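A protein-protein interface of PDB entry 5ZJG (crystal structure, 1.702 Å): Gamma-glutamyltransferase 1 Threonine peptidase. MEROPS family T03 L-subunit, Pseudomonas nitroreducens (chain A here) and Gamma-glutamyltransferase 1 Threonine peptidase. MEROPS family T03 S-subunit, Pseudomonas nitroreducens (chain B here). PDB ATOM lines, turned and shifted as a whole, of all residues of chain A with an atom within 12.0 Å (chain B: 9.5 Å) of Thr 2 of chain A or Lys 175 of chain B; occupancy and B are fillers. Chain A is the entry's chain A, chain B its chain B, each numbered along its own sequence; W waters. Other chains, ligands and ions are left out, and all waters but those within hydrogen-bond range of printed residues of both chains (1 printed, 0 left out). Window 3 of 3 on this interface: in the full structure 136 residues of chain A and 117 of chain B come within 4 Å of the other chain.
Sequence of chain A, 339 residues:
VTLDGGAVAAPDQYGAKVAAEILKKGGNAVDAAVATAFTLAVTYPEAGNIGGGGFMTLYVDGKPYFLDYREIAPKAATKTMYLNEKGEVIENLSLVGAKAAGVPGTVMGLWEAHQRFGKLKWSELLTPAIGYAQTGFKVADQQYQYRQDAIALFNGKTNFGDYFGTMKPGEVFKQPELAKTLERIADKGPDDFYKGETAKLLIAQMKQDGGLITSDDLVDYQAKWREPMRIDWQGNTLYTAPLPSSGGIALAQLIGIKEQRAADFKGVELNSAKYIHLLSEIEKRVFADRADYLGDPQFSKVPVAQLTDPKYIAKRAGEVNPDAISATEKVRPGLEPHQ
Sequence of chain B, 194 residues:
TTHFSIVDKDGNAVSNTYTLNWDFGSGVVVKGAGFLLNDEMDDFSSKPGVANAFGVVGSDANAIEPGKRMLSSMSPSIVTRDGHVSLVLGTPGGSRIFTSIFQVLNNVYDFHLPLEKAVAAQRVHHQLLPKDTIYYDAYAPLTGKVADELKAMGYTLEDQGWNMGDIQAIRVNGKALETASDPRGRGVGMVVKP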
ATOM      1  N   THR A   2      -2.290 -24.992  -9.370  1.00  0.00           N
ATOM      2  CA  THR A   2      -1.032 -24.263  -9.215  1.00  0.00           C
ATOM      3  C   THR A   2      -0.447 -23.909 -10.584  1.00  0.00           C
ATOM      4  O   THR A   2       0.305 -24.689 -11.177  1.00  0.00           O
ATOM      5  CB  THR A   2      -0.004 -25.079  -8.408  1.00  0.00           C
ATOM      6  N   LEU A   3      -0.797 -22.717 -11.065  1.00  0.00           N
ATOM      7  CA  LEU A   3      -0.433 -22.249 -12.391  1.00  0.00           C
ATOM      8  C   LEU A   3       0.977 -21.657 -12.398  1.00  0.00           C
ATOM      9  O   LEU A   3       1.602 -21.439 -11.353  1.00  0.00           O
ATOM     10  CB  LEU A   3      -1.434 -21.191 -12.874  1.00  0.00           C
ATOM     11  CG  LEU A   3      -2.887 -21.629 -13.051  1.00  0.00           C
ATOM     12  CD1 LEU A   3      -3.760 -20.425 -13.433  1.00  0.00           C
ATOM     13  CD2 LEU A   3      -2.992 -22.702 -14.091  1.00  0.00           C
ATOM     14  N   ASP A   4       1.472 -21.381 -13.610  1.00  0.00           N
ATOM     15  CA  ASP A   4       2.745 -20.688 -13.802  1.00  0.00           C
ATOM     16  C   ASP A   4       2.773 -19.301 -13.164  1.00  0.00           C
ATOM     17  O   ASP A   4       3.854 -18.708 -13.062  1.00  0.00           O
ATOM     18  CB  ASP A   4       3.044 -20.553 -15.300  1.00  0.00           C
ATOM     19  CG  ASP A   4       3.683 -21.795 -15.895  1.00  0.00           C
ATOM     20  OD1 ASP A   4       3.969 -22.760 -15.148  1.00  0.00           O
ATOM     21  OD2 ASP A   4       3.910 -21.797 -17.127  1.00  0.00           O
ATOM     22  N   GLY A   5       1.628 -18.777 -12.751  1.00  0.00           N
ATOM     23  CA  GLY A   5       1.537 -17.449 -12.185  1.00  0.00           C
ATOM     24  C   GLY A   5       0.086 -17.003 -12.214  1.00  0.00           C
ATOM     25  O   GLY A   5      -0.822 -17.806 -12.413  1.00  0.00           O
ATOM     26  N   GLY A   6      -0.109 -15.705 -11.993  1.00  0.00           N
ATOM     27  CA  GLY A   6      -1.395 -15.076 -12.174  1.00  0.00           C
ATOM     28  C   GLY A   6      -1.380 -14.169 -13.391  1.00  0.00           C
ATOM     29  O   GLY A   6      -0.385 -14.043 -14.098  1.00  0.00           O
ATOM     30  N   ALA A   7      -2.516 -13.502 -13.615  1.00  0.00           N
ATOM     31  CA  ALA A   7      -2.562 -12.610 -14.759  1.00  0.00           C
ATOM     32  C   ALA A   7      -3.705 -11.623 -14.607  1.00  0.00           C
ATOM     33  O   ALA A   7      -4.679 -11.878 -13.895  1.00  0.00           O
ATOM     34  CB  ALA A   7      -2.706 -13.402 -16.068  1.00  0.00           C
ATOM     35  N   VAL A   8      -3.551 -10.472 -15.249  1.00  0.00           N
ATOM     36  CA  VAL A   8      -4.608  -9.467 -15.309  1.00  0.00           C
ATOM     37  C   VAL A   8      -4.708  -8.957 -16.738  1.00  0.00           C
ATOM     38  O   VAL A   8      -3.699  -8.815 -17.435  1.00  0.00           O
ATOM     39  CB  VAL A   8      -4.378  -8.288 -14.338  1.00  0.00           C
ATOM     40  CG1 VAL A   8      -2.993  -7.705 -14.482  1.00  0.00           C
ATOM     41  CG2 VAL A   8      -5.428  -7.200 -14.544  1.00  0.00           C
ATOM     42  N   TYR A  59     -14.747 -17.664 -10.052  1.00  0.00           N
ATOM     43  CA  TYR A  59     -14.509 -19.094  -9.930  1.00  0.00           C
ATOM     44  C   TYR A  59     -13.458 -19.236  -8.843  1.00  0.00           C
ATOM     45  O   TYR A  59     -12.333 -18.777  -9.024  1.00  0.00           O
ATOM     46  CB  TYR A  59     -14.033 -19.688 -11.252  1.00  0.00           C
ATOM     47  CG  TYR A  59     -14.202 -21.183 -11.322  1.00  0.00           C
ATOM     48  CD1 TYR A  59     -15.455 -21.735 -11.521  1.00  0.00           C
ATOM     49  CD2 TYR A  59     -13.120 -22.036 -11.183  1.00  0.00           C
ATOM     50  CE1 TYR A  59     -15.637 -23.103 -11.577  1.00  0.00           C
ATOM     51  CE2 TYR A  59     -13.294 -23.413 -11.243  1.00  0.00           C
ATOM     52  CZ  TYR A  59     -14.559 -23.934 -11.438  1.00  0.00           C
ATOM     53  OH  TYR A  59     -14.753 -25.299 -11.495  1.00  0.00           O
ATOM     54  N   VAL A  60     -13.836 -19.809  -7.700  1.00  0.00           N
ATOM     55  CA  VAL A  60     -12.974 -19.833  -6.520  1.00  0.00           C
ATOM     56  C   VAL A  60     -12.982 -21.247  -5.966  1.00  0.00           C
ATOM     57  O   VAL A  60     -14.049 -21.781  -5.645  1.00  0.00           O
ATOM     58  CB  VAL A  60     -13.436 -18.840  -5.442  1.00  0.00           C
ATOM     59  CG1 VAL A  60     -12.514 -18.909  -4.233  1.00  0.00           C
ATOM     60  CG2 VAL A  60     -13.495 -17.408  -6.006  1.00  0.00           C
ATOM     61  N   ASP A  61     -11.795 -21.837  -5.839  1.00  0.00           N
ATOM     62  CA  ASP A  61     -11.641 -23.203  -5.342  1.00  0.00           C
ATOM     63  C   ASP A  61     -12.607 -24.158  -6.040  1.00  0.00           C
ATOM     64  O   ASP A  61     -13.307 -24.949  -5.407  1.00  0.00           O
ATOM     65  CB  ASP A  61     -11.822 -23.240  -3.823  1.00  0.00           C
ATOM     66  CG  ASP A  61     -10.816 -22.363  -3.105  1.00  0.00           C
ATOM     67  OD1 ASP A  61      -9.685 -22.223  -3.619  1.00  0.00           O
ATOM     68  OD2 ASP A  61     -11.154 -21.805  -2.039  1.00  0.00           O
ATOM     69  N   GLY A  62     -12.633 -24.080  -7.370  1.00  0.00           N
ATOM     70  CA  GLY A  62     -13.431 -24.998  -8.164  1.00  0.00           C
ATOM     71  C   GLY A  62     -14.928 -24.792  -8.111  1.00  0.00           C
ATOM     72  O   GLY A  62     -15.677 -25.700  -8.480  1.00  0.00           O
ATOM     73  N   VAL B   7      -6.857 -13.740 -13.112  1.00  0.00           N
ATOM     74  CA  VAL B   7      -6.657 -15.121 -12.692  1.00  0.00           C
ATOM     75  C   VAL B   7      -5.498 -15.117 -11.713  1.00  0.00           C
ATOM     76  O   VAL B   7      -4.479 -14.469 -11.972  1.00  0.00           O
ATOM     77  CB  VAL B   7      -6.347 -16.038 -13.897  1.00  0.00           C
ATOM     78  CG1 VAL B   7      -5.988 -17.444 -13.447  1.00  0.00           C
ATOM     79  CG2 VAL B   7      -7.533 -16.108 -14.827  1.00  0.00           C
ATOM     80  N   ASP B   8      -5.628 -15.839 -10.600  1.00  0.00           N
ATOM     81  CA  ASP B   8      -4.489 -15.941  -9.695  1.00  0.00           C
ATOM     82  C   ASP B   8      -3.791 -17.294  -9.849  1.00  0.00           C
ATOM     83  O   ASP B   8      -4.226 -18.170 -10.600  1.00  0.00           O
ATOM     84  CB  ASP B   8      -4.893 -15.649  -8.233  1.00  0.00           C
ATOM     85  CG  ASP B   8      -5.802 -16.704  -7.599  1.00  0.00           C
ATOM     86  OD1 ASP B   8      -5.757 -17.890  -7.965  1.00  0.00           O
ATOM     87  OD2 ASP B   8      -6.562 -16.315  -6.678  1.00  0.00           O
ATOM     88  N   LYS B   9      -2.649 -17.426  -9.168  1.00  0.00           N
ATOM     89  CA  LYS B   9      -1.784 -18.589  -9.345  1.00  0.00           C
ATOM     90  C   LYS B   9      -2.417 -19.872  -8.828  1.00  0.00           C
ATOM     91  O   LYS B   9      -1.910 -20.958  -9.131  1.00  0.00           O
ATOM     92  CB  LYS B   9      -0.438 -18.368  -8.650  1.00  0.00           C
ATOM     93  CG  LYS B   9      -0.501 -18.280  -7.132  1.00  0.00           C
ATOM     94  CD  LYS B   9       0.878 -17.992  -6.561  1.00  0.00           C
ATOM     95  CE  LYS B   9       0.850 -17.876  -5.049  1.00  0.00           C
ATOM     96  NZ  LYS B   9       0.000 -16.724  -4.601  1.00  0.00           N
ATOM     97  N   ASP B  10      -3.502 -19.768  -8.062  1.00  0.00           N
ATOM     98  CA  ASP B  10      -4.249 -20.920  -7.587  1.00  0.00           C
ATOM     99  C   ASP B  10      -5.367 -21.315  -8.545  1.00  0.00           C
ATOM    100  O   ASP B  10      -6.131 -22.229  -8.235  1.00  0.00           O
ATOM    101  CB  ASP B  10      -4.834 -20.623  -6.206  1.00  0.00           C
ATOM    102  CG  ASP B  10      -3.759 -20.430  -5.145  1.00  0.00           C
ATOM    103  OD1 ASP B  10      -2.806 -21.227  -5.112  1.00  0.00           O
ATOM    104  OD2 ASP B  10      -3.870 -19.476  -4.348  1.00  0.00           O
ATOM    105  N   GLY B  11      -5.470 -20.661  -9.695  1.00  0.00           N
ATOM    106  CA  GLY B  11      -6.528 -20.965 -10.640  1.00  0.00           C
ATOM    107  C   GLY B  11      -7.860 -20.316 -10.345  1.00  0.00           C
ATOM    108  O   GLY B  11      -8.856 -20.657 -11.005  1.00  0.00           O
ATOM    109  N   ASN B  12      -7.928 -19.422  -9.361  1.00  0.00           N
ATOM    110  CA  ASN B  12      -9.153 -18.672  -9.121  1.00  0.00           C
ATOM    111  C   ASN B  12      -9.245 -17.519 -10.115  1.00  0.00           C
ATOM    112  O   ASN B  12      -8.237 -16.985 -10.578  1.00  0.00           O
ATOM    113  CB  ASN B  12      -9.211 -18.135  -7.691  1.00  0.00           C
ATOM    114  CG  ASN B  12      -8.976 -19.197  -6.655  1.00  0.00           C
ATOM    115  OD1 ASN B  12      -9.584 -20.270  -6.692  1.00  0.00           O
ATOM    116  ND2 ASN B  12      -8.066 -18.916  -5.723  1.00  0.00           N
ATOM    117  N   HIS B  84     -11.479 -26.578 -14.527  1.00  0.00           N
ATOM    118  CA  HIS B  84     -10.392 -25.614 -14.445  1.00  0.00           C
ATOM    119  C   HIS B  84     -10.672 -24.427 -15.354  1.00  0.00           C
ATOM    120  O   HIS B  84     -11.098 -24.587 -16.504  1.00  0.00           O
ATOM    121  CB  HIS B  84      -9.065 -26.263 -14.822  1.00  0.00           C
ATOM    122  CG  HIS B  84      -8.671 -27.393 -13.920  1.00  0.00           C
ATOM    123  ND1 HIS B  84      -8.316 -27.203 -12.602  1.00  0.00           N
ATOM    124  CD2 HIS B  84      -8.584 -28.726 -14.143  1.00  0.00           C
ATOM    125  CE1 HIS B  84      -8.020 -28.368 -12.052  1.00  0.00           C
ATOM    126  NE2 HIS B  84      -8.175 -29.308 -12.966  1.00  0.00           N
ATOM    127  N   VAL B  85     -10.416 -23.228 -14.830  1.00  0.00           N
ATOM    128  CA  VAL B  85     -10.546 -22.031 -15.641  1.00  0.00           C
ATOM    129  C   VAL B  85      -9.737 -22.198 -16.912  1.00  0.00           C
ATOM    130  O   VAL B  85      -8.564 -22.604 -16.881  1.00  0.00           O
ATOM    131  CB  VAL B  85     -10.106 -20.792 -14.844  1.00  0.00           C
ATOM    132  CG1 VAL B  85     -10.102 -19.573 -15.737  1.00  0.00           C
ATOM    133  CG2 VAL B  85     -11.041 -20.565 -13.654  1.00  0.00           C
ATOM    134  N   ILE B 170      -8.231 -13.332 -20.560  1.00  0.00           N
ATOM    135  CA  ILE B 170      -7.118 -14.165 -20.105  1.00  0.00           C
ATOM    136  C   ILE B 170      -7.399 -15.583 -20.568  1.00  0.00           C
ATOM    137  O   ILE B 170      -8.496 -16.093 -20.345  1.00  0.00           O
ATOM    138  CB  ILE B 170      -6.971 -14.144 -18.570  1.00  0.00           C
ATOM    139  CG1 ILE B 170      -6.607 -12.740 -18.078  1.00  0.00           C
ATOM    140  CG2 ILE B 170      -5.914 -15.165 -18.105  1.00  0.00           C
ATOM    141  CD1 ILE B 170      -6.713 -12.599 -16.577  1.00  0.00           C
ATOM    142  N   ARG B 171      -6.414 -16.229 -21.202  1.00  0.00           N
ATOM    143  CA  ARG B 171      -6.550 -17.633 -21.569  1.00  0.00           C
ATOM    144  C   ARG B 171      -5.558 -18.463 -20.765  1.00  0.00           C
ATOM    145  O   ARG B 171      -4.408 -18.054 -20.571  1.00  0.00           O
ATOM    146  CB  ARG B 171      -6.331 -17.860 -23.072  1.00  0.00           C
ATOM    147  CG  ARG B 171      -6.402 -19.325 -23.431  1.00  0.00           C
ATOM    148  CD  ARG B 171      -6.892 -19.582 -24.840  1.00  0.00           C
ATOM    149  NE  ARG B 171      -5.984 -19.078 -25.863  1.00  0.00           N
ATOM    150  CZ  ARG B 171      -6.080 -19.366 -27.158  1.00  0.00           C
ATOM    151  NH1 ARG B 171      -7.048 -20.170 -27.600  1.00  0.00           N
ATOM    152  NH2 ARG B 171      -5.200 -18.853 -28.015  1.00  0.00           N
ATOM    153  N   VAL B 172      -6.010 -19.618 -20.276  1.00  0.00           N
ATOM    154  CA  VAL B 172      -5.175 -20.526 -19.494  1.00  0.00           C
ATOM    155  C   VAL B 172      -5.009 -21.796 -20.302  1.00  0.00           C
ATOM    156  O   VAL B 172      -6.000 -22.369 -20.768  1.00  0.00           O
ATOM    157  CB  VAL B 172      -5.779 -20.838 -18.113  1.00  0.00           C
ATOM    158  CG1 VAL B 172      -4.877 -21.817 -17.336  1.00  0.00           C
ATOM    159  CG2 VAL B 172      -5.997 -19.548 -17.314  1.00  0.00           C
ATOM    160  N   ASN B 173      -3.761 -22.235 -20.468  1.00  0.00           N
ATOM    161  CA  ASN B 173      -3.435 -23.381 -21.312  1.00  0.00           C
ATOM    162  C   ASN B 173      -2.561 -24.290 -20.460  1.00  0.00           C
ATOM    163  O   ASN B 173      -1.343 -24.102 -20.372  1.00  0.00           O
ATOM    164  CB  ASN B 173      -2.753 -22.940 -22.601  1.00  0.00           C
ATOM    165  CG  ASN B 173      -3.561 -21.885 -23.357  1.00  0.00           C
ATOM    166  OD1 ASN B 173      -3.286 -20.684 -23.253  1.00  0.00           O
ATOM    167  ND2 ASN B 173      -4.567 -22.328 -24.114  1.00  0.00           N
ATOM    168  N   GLY B 174      -3.183 -25.263 -19.822  1.00  0.00           N
ATOM    169  CA  GLY B 174      -2.460 -26.034 -18.829  1.00  0.00           C
ATOM    170  C   GLY B 174      -2.073 -25.115 -17.691  1.00  0.00           C
ATOM    171  O   GLY B 174      -2.928 -24.493 -17.047  1.00  0.00           O
ATOM    172  N   LYS B 175      -0.770 -24.986 -17.452  1.00  0.00           N
ATOM    173  CA  LYS B 175      -0.281 -24.084 -16.418  1.00  0.00           C
ATOM    174  C   LYS B 175       0.040 -22.684 -16.933  1.00  0.00           C
ATOM    175  O   LYS B 175       0.254 -21.783 -16.119  1.00  0.00           O
ATOM    176  CB  LYS B 175       0.968 -24.678 -15.751  1.00  0.00           C
ATOM    177  CG  LYS B 175       0.657 -25.817 -14.791  1.00  0.00           C
ATOM    178  N   ALA B 176       0.093 -22.482 -18.247  1.00  0.00           N
ATOM    179  CA  ALA B 176       0.495 -21.207 -18.830  1.00  0.00           C
ATOM    180  C   ALA B 176      -0.692 -20.262 -18.971  1.00  0.00           C
ATOM    181  O   ALA B 176      -1.833 -20.692 -19.152  1.00  0.00           O
ATOM    182  CB  ALA B 176       1.124 -21.426 -20.206  1.00  0.00           C
ATOM    183  N   LEU B 177      -0.406 -18.962 -18.911  1.00  0.00           N
ATOM    184  CA  LEU B 177      -1.429 -17.930 -19.066  1.00  0.00           C
ATOM    185  C   LEU B 177      -1.011 -16.943 -20.148  1.00  0.00           C
ATOM    186  O   LEU B 177       0.178 -16.697 -20.358  1.00  0.00           O
ATOM    187  CB  LEU B 177      -1.663 -17.166 -17.755  1.00  0.00           C
ATOM    188  CG  LEU B 177      -2.011 -17.990 -16.515  1.00  0.00           C
ATOM    189  CD1 LEU B 177      -0.751 -18.491 -15.814  1.00  0.00           C
ATOM    190  CD2 LEU B 177      -2.854 -17.171 -15.568  1.00  0.00           C
ATOM    191  N   GLU B 178      -2.002 -16.380 -20.839  1.00  0.00           N
ATOM    192  CA  GLU B 178      -1.793 -15.306 -21.797  1.00  0.00           C
ATOM    193  C   GLU B 178      -2.919 -14.300 -21.630  1.00  0.00           C
ATOM    194  O   GLU B 178      -4.023 -14.658 -21.219  1.00  0.00           O
ATOM    195  CB  GLU B 178      -1.764 -15.807 -23.249  1.00  0.00           C
ATOM    196  CG  GLU B 178      -3.074 -16.438 -23.708  1.00  0.00           C
ATOM    197  CD  GLU B 178      -3.050 -16.939 -25.141  1.00  0.00           C
ATOM    198  OE1 GLU B 178      -2.462 -16.271 -26.016  1.00  0.00           O
ATOM    199  OE2 GLU B 178      -3.633 -18.013 -25.394  1.00  0.00           O
ATOM    200  N   VAL B 191       1.225 -10.946 -17.092  1.00  0.00           N
ATOM    201  CA  VAL B 191       1.349 -12.200 -16.363  1.00  0.00           C
ATOM    202  C   VAL B 191       2.342 -11.961 -15.239  1.00  0.00           C
ATOM    203  O   VAL B 191       3.373 -11.301 -15.434  1.00  0.00           O
ATOM    204  CB  VAL B 191       1.788 -13.364 -17.276  1.00  0.00           C
ATOM    205  CG1 VAL B 191       1.772 -14.686 -16.504  1.00  0.00           C
ATOM    206  CG2 VAL B 191       0.879 -13.448 -18.495  1.00  0.00           C
ATOM    207  N   VAL B 192       2.023 -12.482 -14.061  1.00  0.00           N
ATOM    208  CA  VAL B 192       2.777 -12.234 -12.839  1.00  0.00           C
ATOM    209  C   VAL B 192       3.276 -13.573 -12.302  1.00  0.00           C
ATOM    210  O   VAL B 192       2.480 -14.444 -11.938  1.00  0.00           O
ATOM    211  CB  VAL B 192       1.920 -11.481 -11.804  1.00  0.00           C
ATOM    212  CG1 VAL B 192       0.588 -12.139 -11.623  1.00  0.00           C
ATOM    213  CG2 VAL B 192       2.620 -11.364 -10.501  1.00  0.00           C
ATOM    214  N   PRO B 194       4.621 -16.367  -9.764  1.00  0.00           N
ATOM    215  CA  PRO B 194       4.153 -16.569  -8.392  1.00  0.00           C
ATOM    216  C   PRO B 194       5.128 -15.995  -7.381  1.00  0.00           C
ATOM    217  O   PRO B 194       4.770 -15.130  -6.582  1.00  0.00           O
ATOM    218  CB  PRO B 194       4.051 -18.091  -8.275  1.00  0.00           C
ATOM    219  CG  PRO B 194       4.963 -18.617  -9.317  1.00  0.00           C
ATOM    220  CD  PRO B 194       4.930 -17.638 -10.435  1.00  0.00           C
ATOM    221  OXT PRO B 194       6.300 -16.361  -7.361  1.00  0.00           O
HETATM  222  O   HOH W   1     -10.396 -22.516  -8.625  1.00  0.00           O
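Among the printed residues, pairs that only touch across the chains: Thr 2 of chain A with Lys 9 of chain B, Thr 2 of chain A with Lys 175 of chain B, Leu 3 of chain A with Val 7 of chain B, Leu 3 of chain A with Asp 8 of chain B, Leu 3 of chain A with Gly 11 of chain B, Leu 3 of chain A with Val 172 of chain B, Leu 3 of chain A with Gly 174 of chain B, Leu 3 of chain A with Lys 175 of chain B, Leu 3 of chain A with Leu 177 of chain B, Asp 4 of chain A with Ala 176 of chain B, Asp 4 of chain A with Pro 194 of chain B, Gly 5 of chain A with Asp 8 of chain B, Gly 5 of chain A with Lys 9 of chain B, Gly 5 of chain A with Leu 177 of chain B, Gly 5 of chain A with Val 192 of chain B, Gly 5 of chain A with Pro 194 of chain B, Gly 6 of chain A with Val 7 of chain B, Gly 6 of chain A with Leu 177 of chain B, Gly 6 of chain A with Val 191 of chain B, Ala 7 of chain A with Ile 170 of chain B, Ala 7 of chain A with Leu 177 of chain B, Ala 7 of chain A with Val 192 of chain B, Val 8 of chain A with Ile 170 of chain B, Tyr 59 of chain A with Asn 12 of chain B, Tyr 59 of chain A with Val 85 of chain B and Val 60 of chain A with Asn 12 of chain B.
The backbone NH (N) of Leu 3 of chain A lies within hydrogen-bond range of the backbone carbonyl oxygen (O) of Lys 9 of chain B, 2.8 Å away.
The backbone carbonyl oxygen (O) of Lys 175 of chain B sits at hydrogen-bond distance from the backbone NH (N) of Asp 4 of chain A, at 2.8 Å.
The backbone carbonyl oxygen of Gly 6 of chain A lies within hydrogen-bond range of the backbone NH of Val 192 of chain B (2.9 Å).
N of Ala 7 of chain A lies within hydrogen-bond range of O of Val 7 of chain B (2.7 Å).
The backbone NH (N) of Asp 61 of chain A lies within hydrogen-bond range of the side-chain amide oxygen (OD1) of Asn 12 of chain B, 2.8 Å away.
Printed residues of chain A that touch a printed residue of chain B: Thr 2, Leu 3, Asp 4, Gly 5, Gly 6, Ala 7, Val 8, Tyr 59, Val 60 and Asp 61.
Hydrophobic or aromatic side chains of chain A that line the printed part of chain B: Leu 3, Ala 7 and Tyr 59.
Along chain A the printed residues that touch a printed residue of chain B span positions 2 to 61.
Of the 20 printed residues of chain B, 15 touch a printed residue of chain A.
Printed residues of chain B within 4 Å of Val 60 of chain A: Asn 12.
Gly 62 of chain A touches none of the printed residues of chain B.
Of the printed residues of chain A, Val 7 of chain B touches Leu 3 (3.7 Å), Gly 6 (3.1 Å) and Ala 7 (2.7 Å).
No residue of chain A comes within 4 Å of Asp 10 of chain B.
Printed residues of chain A within 4 Å of Val 85 of chain B: Tyr 59 (3.5 Å).
Arg 171 of chain B touches none of the printed residues of chain A.
Of chain A, only Leu 3 comes within 4 Å of Val 172 of chain B.
Of chain A, only Leu 3 comes within 4 Å of Gly 174 of chain B.
Lys 175 of chain B touches just these residues of chain A: Thr 2 (3.8 Å), Leu 3 (3.7 Å) and Asp 4 (2.8 Å).
Ala 176 of chain B touches one residue of chain A.
The nearest residue of chain B that does not touch Thr 2 of chain A is Asp 10 of chain B (4.9 Å).
The nearest residue of chain A that does not touch Lys 175 of chain B is Gly 5 of chain A (4.7 Å).
The backbone carbonyl oxygen (O) of Gly 62 of chain A lies within hydrogen-bond range of the side-chain hydroxyl (OH) of Tyr 59 of chain A (3.2 Å).
The backbone NH of Asp 10 of chain B lies within hydrogen-bond range of the side-chain carboxylate of Asp 8 of chain B, at 2.9 Å.
The backbone NH of Gly 11 of chain B sits at hydrogen-bond distance from the side-chain carboxylate of Asp 8 of chain B.
OD1 of Asp 8 of chain B sits at hydrogen-bond distance from N of Asn 12 of chain B, at 3.0 Å.
Water W1 lies within hydrogen-bond range of the backbone NH of Gly 62 of chain A, the side-chain amide oxygen of Asn 12 of chain B, the backbone NH of Asp 61 of chain A and the backbone carbonyl oxygen of Gly 11 of chain B.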
